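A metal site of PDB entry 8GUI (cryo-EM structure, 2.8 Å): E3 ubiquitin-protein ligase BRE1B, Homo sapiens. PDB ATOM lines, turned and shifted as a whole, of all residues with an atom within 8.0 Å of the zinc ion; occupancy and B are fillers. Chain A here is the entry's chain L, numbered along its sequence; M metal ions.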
ATOM      1  N   LEU A 960      -4.251  -3.213 -21.921  1.00  0.00           N
ATOM      2  CA  LEU A 960      -4.258  -4.463 -22.669  1.00  0.00           C
ATOM      3  C   LEU A 960      -4.619  -5.602 -21.723  1.00  0.00           C
ATOM      4  O   LEU A 960      -3.936  -5.812 -20.716  1.00  0.00           O
ATOM      5  CB  LEU A 960      -2.899  -4.719 -23.324  1.00  0.00           C
ATOM      6  CG  LEU A 960      -2.467  -3.761 -24.437  1.00  0.00           C
ATOM      7  CD1 LEU A 960      -1.050  -4.065 -24.876  1.00  0.00           C
ATOM      8  CD2 LEU A 960      -3.429  -3.841 -25.603  1.00  0.00           C
ATOM      9  N   LYS A 962      -4.430  -8.781 -21.960  1.00  0.00           N
ATOM     10  CA  LYS A 962      -3.609  -9.985 -21.983  1.00  0.00           C
ATOM     11  C   LYS A 962      -2.182  -9.740 -21.496  1.00  0.00           C
ATOM     12  O   LYS A 962      -1.377 -10.678 -21.482  1.00  0.00           O
ATOM     13  CB  LYS A 962      -3.576 -10.596 -23.383  1.00  0.00           C
ATOM     14  CG  LYS A 962      -4.798 -11.445 -23.761  1.00  0.00           C
ATOM     15  CD  LYS A 962      -6.045 -10.609 -24.025  1.00  0.00           C
ATOM     16  CE  LYS A 962      -7.203 -11.489 -24.475  1.00  0.00           C
ATOM     17  NZ  LYS A 962      -8.465 -10.714 -24.631  1.00  0.00           N
ATOM     18  N   CYS A 963      -1.850  -8.519 -21.101  1.00  0.00           N
ATOM     19  CA  CYS A 963      -0.536  -8.227 -20.533  1.00  0.00           C
ATOM     20  C   CYS A 963      -0.584  -7.307 -19.323  1.00  0.00           C
ATOM     21  O   CYS A 963       0.483  -7.034 -18.753  1.00  0.00           O
ATOM     22  CB  CYS A 963       0.384  -7.601 -21.593  1.00  0.00           C
ATOM     23  SG  CYS A 963       0.156  -5.836 -21.822  1.00  0.00           S
ATOM     24  N   PHE A 964      -1.766  -6.836 -18.923  1.00  0.00           N
ATOM     25  CA  PHE A 964      -1.959  -6.121 -17.659  1.00  0.00           C
ATOM     26  C   PHE A 964      -1.153  -4.818 -17.602  1.00  0.00           C
ATOM     27  O   PHE A 964      -0.644  -4.425 -16.556  1.00  0.00           O
ATOM     28  CB  PHE A 964      -1.619  -7.020 -16.465  1.00  0.00           C
ATOM     29  CG  PHE A 964      -2.758  -7.888 -16.009  1.00  0.00           C
ATOM     30  CD1 PHE A 964      -3.827  -8.163 -16.844  1.00  0.00           C
ATOM     31  CD2 PHE A 964      -2.739  -8.451 -14.749  1.00  0.00           C
ATOM     32  CE1 PHE A 964      -4.856  -8.974 -16.435  1.00  0.00           C
ATOM     33  CE2 PHE A 964      -3.775  -9.270 -14.318  1.00  0.00           C
ATOM     34  CZ  PHE A 964      -4.834  -9.526 -15.166  1.00  0.00           C
ATOM     35  N   HIS A 965      -1.034  -4.137 -18.745  1.00  0.00           N
ATOM     36  CA  HIS A 965      -0.285  -2.902 -18.836  1.00  0.00           C
ATOM     37  C   HIS A 965      -1.184  -1.786 -19.354  1.00  0.00           C
ATOM     38  O   HIS A 965      -2.113  -2.018 -20.129  1.00  0.00           O
ATOM     39  CB  HIS A 965       0.930  -3.046 -19.755  1.00  0.00           C
ATOM     40  CG  HIS A 965       1.884  -4.115 -19.343  1.00  0.00           C
ATOM     41  ND1 HIS A 965       2.335  -5.093 -20.204  1.00  0.00           N
ATOM     42  CD2 HIS A 965       2.477  -4.363 -18.151  1.00  0.00           C
ATOM     43  CE1 HIS A 965       3.167  -5.901 -19.568  1.00  0.00           C
ATOM     44  NE2 HIS A 965       3.268  -5.485 -18.316  1.00  0.00           N
ATOM     45  N   VAL A 966      -0.894  -0.558 -18.920  1.00  0.00           N
ATOM     46  CA  VAL A 966      -1.714   0.599 -19.222  1.00  0.00           C
ATOM     47  C   VAL A 966      -1.075   1.364 -20.375  1.00  0.00           C
ATOM     48  O   VAL A 966       0.118   1.694 -20.327  1.00  0.00           O
ATOM     49  CB  VAL A 966      -1.873   1.510 -17.998  1.00  0.00           C
ATOM     50  CG1 VAL A 966      -2.959   2.555 -18.237  1.00  0.00           C
ATOM     51  CG2 VAL A 966      -2.153   0.690 -16.762  1.00  0.00           C
ATOM     52  N   PHE A 967      -1.860   1.641 -21.417  1.00  0.00           N
ATOM     53  CA  PHE A 967      -1.401   2.423 -22.554  1.00  0.00           C
ATOM     54  C   PHE A 967      -2.422   3.494 -22.891  1.00  0.00           C
ATOM     55  O   PHE A 967      -3.392   3.692 -22.160  1.00  0.00           O
ATOM     56  CB  PHE A 967      -1.157   1.516 -23.765  1.00  0.00           C
ATOM     57  CG  PHE A 967       0.081   0.689 -23.653  1.00  0.00           C
ATOM     58  CD1 PHE A 967       1.262   1.227 -23.165  1.00  0.00           C
ATOM     59  CD2 PHE A 967       0.069  -0.650 -24.026  1.00  0.00           C
ATOM     60  CE1 PHE A 967       2.400   0.458 -23.067  1.00  0.00           C
ATOM     61  CE2 PHE A 967       1.209  -1.419 -23.918  1.00  0.00           C
ATOM     62  CZ  PHE A 967       2.380  -0.860 -23.439  1.00  0.00           C
ATOM     63  N   LYS A 982       1.765  -6.516 -31.405  1.00  0.00           N
ATOM     64  CA  LYS A 982       2.810  -6.670 -30.415  1.00  0.00           C
ATOM     65  C   LYS A 982       2.644  -5.581 -29.365  1.00  0.00           C
ATOM     66  O   LYS A 982       2.444  -4.413 -29.705  1.00  0.00           O
ATOM     67  CB  LYS A 982       4.210  -6.575 -31.050  1.00  0.00           C
ATOM     68  CG  LYS A 982       4.561  -7.631 -32.110  1.00  0.00           C
ATOM     69  CD  LYS A 982       4.809  -9.025 -31.521  1.00  0.00           C
ATOM     70  CE  LYS A 982       3.587  -9.936 -31.557  1.00  0.00           C
ATOM     71  NZ  LYS A 982       3.885 -11.314 -31.081  1.00  0.00           N
ATOM     72  N   CYS A 983       2.715  -5.967 -28.097  1.00  0.00           N
ATOM     73  CA  CYS A 983       2.615  -4.983 -27.023  1.00  0.00           C
ATOM     74  C   CYS A 983       3.860  -4.097 -27.011  1.00  0.00           C
ATOM     75  O   CYS A 983       4.982  -4.591 -27.141  1.00  0.00           O
ATOM     76  CB  CYS A 983       2.444  -5.673 -25.675  1.00  0.00           C
ATOM     77  SG  CYS A 983       2.640  -4.558 -24.272  1.00  0.00           S
ATOM     78  N   PRO A 984       3.691  -2.780 -26.865  1.00  0.00           N
ATOM     79  CA  PRO A 984       4.872  -1.916 -26.705  1.00  0.00           C
ATOM     80  C   PRO A 984       5.710  -2.233 -25.478  1.00  0.00           C
ATOM     81  O   PRO A 984       6.912  -1.947 -25.469  1.00  0.00           O
ATOM     82  CB  PRO A 984       4.249  -0.513 -26.613  1.00  0.00           C
ATOM     83  CG  PRO A 984       2.946  -0.616 -27.328  1.00  0.00           C
ATOM     84  CD  PRO A 984       2.456  -2.013 -27.087  1.00  0.00           C
ATOM     85  N   LYS A 985       5.109  -2.818 -24.435  1.00  0.00           N
ATOM     86  CA  LYS A 985       5.838  -3.115 -23.207  1.00  0.00           C
ATOM     87  C   LYS A 985       6.398  -4.534 -23.192  1.00  0.00           C
ATOM     88  O   LYS A 985       7.609  -4.734 -23.083  1.00  0.00           O
ATOM     89  CB  LYS A 985       4.926  -2.884 -21.998  1.00  0.00           C
ATOM     90  CG  LYS A 985       5.588  -3.155 -20.655  1.00  0.00           C
ATOM     91  CD  LYS A 985       6.551  -2.042 -20.282  1.00  0.00           C
ATOM     92  CE  LYS A 985       7.106  -2.250 -18.890  1.00  0.00           C
ATOM     93  NZ  LYS A 985       6.040  -2.180 -17.854  1.00  0.00           N
ATOM     94  N   CYS A 986       5.522  -5.542 -23.294  1.00  0.00           N
ATOM     95  CA  CYS A 986       5.911  -6.933 -23.123  1.00  0.00           C
ATOM     96  C   CYS A 986       5.771  -7.751 -24.403  1.00  0.00           C
ATOM     97  O   CYS A 986       5.938  -8.971 -24.360  1.00  0.00           O
ATOM     98  CB  CYS A 986       5.106  -7.574 -21.994  1.00  0.00           C
ATOM     99  SG  CYS A 986       3.352  -7.768 -22.353  1.00  0.00           S
ATOM    100  N   ASN A 987       5.437  -7.118 -25.530  1.00  0.00           N
ATOM    101  CA  ASN A 987       5.341  -7.761 -26.841  1.00  0.00           C
ATOM    102  C   ASN A 987       4.313  -8.891 -26.872  1.00  0.00           C
ATOM    103  O   ASN A 987       4.371  -9.764 -27.750  1.00  0.00           O
ATOM    104  CB  ASN A 987       6.699  -8.275 -27.315  1.00  0.00           C
ATOM    105  CG  ASN A 987       7.742  -7.176 -27.398  1.00  0.00           C
ATOM    106  OD1 ASN A 987       8.371  -6.828 -26.394  1.00  0.00           O
ATOM    107  ND2 ASN A 987       7.932  -6.616 -28.588  1.00  0.00           N
ATOM    108  N   ALA A 988       3.360  -8.890 -25.947  1.00  0.00           N
ATOM    109  CA  ALA A 988       2.319  -9.915 -25.942  1.00  0.00           C
ATOM    110  C   ALA A 988       1.329  -9.657 -27.073  1.00  0.00           C
ATOM    111  O   ALA A 988       0.996  -8.515 -27.393  1.00  0.00           O
ATOM    112  CB  ALA A 988       1.591  -9.941 -24.602  1.00  0.00           C
ATOM    113  N   ALA A 989       0.855 -10.743 -27.683  1.00  0.00           N
ATOM    114  CA  ALA A 989      -0.118 -10.633 -28.756  1.00  0.00           C
ATOM    115  C   ALA A 989      -1.471 -10.205 -28.216  1.00  0.00           C
ATOM    116  O   ALA A 989      -1.894 -10.623 -27.139  1.00  0.00           O
ATOM    117  CB  ALA A 989      -0.246 -11.962 -29.505  1.00  0.00           C
ATOM    118  N   PHE A 990      -2.158  -9.340 -28.977  1.00  0.00           N
ATOM    119  CA  PHE A 990      -3.479  -8.878 -28.599  1.00  0.00           C
ATOM    120  C   PHE A 990      -4.260  -8.529 -29.860  1.00  0.00           C
ATOM    121  O   PHE A 990      -3.681  -8.296 -30.927  1.00  0.00           O
ATOM    122  CB  PHE A 990      -3.427  -7.686 -27.641  1.00  0.00           C
ATOM    123  CG  PHE A 990      -2.715  -6.486 -28.203  1.00  0.00           C
ATOM    124  CD1 PHE A 990      -1.337  -6.383 -28.138  1.00  0.00           C
ATOM    125  CD2 PHE A 990      -3.430  -5.452 -28.786  1.00  0.00           C
ATOM    126  CE1 PHE A 990      -0.677  -5.275 -28.653  1.00  0.00           C
ATOM    127  CE2 PHE A 990      -2.782  -4.345 -29.308  1.00  0.00           C
ATOM    128  CZ  PHE A 990      -1.403  -4.260 -29.232  1.00  0.00           C
HETATM  129 ZN    ZN M   1       2.435  -5.631 -22.227  1.00  0.00          ZN
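Merely in contact with the zinc ion: Lys 985 (3.7 Å).
Of the 16 residues printed, 5 come within 4 Å of the zinc ion.
The nearest printed residue that does not touch the zinc ion is Leu 960 (4.6 Å).
The zinc ion is bound by ND1 of His 965 (2.1 Å).
SG of Cys 983 binds the zinc ion (2.3 Å).
SG of Cys 963 binds the zinc ion, 2.3 Å away.
SG of Cys 986 binds the zinc ion, at 2.3 Å.
O of His 965 sits at hydrogen-bond distance from N of Leu 960.
SG of Cys 983 sits close to N of Lys 985, 3.0 Å away.
N of Cys 983 sits at hydrogen-bond distance from O of Ala 988, at 3.2 Å.
SG of Cys 986 lies close to N of Ala 988, at 3.8 Å.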
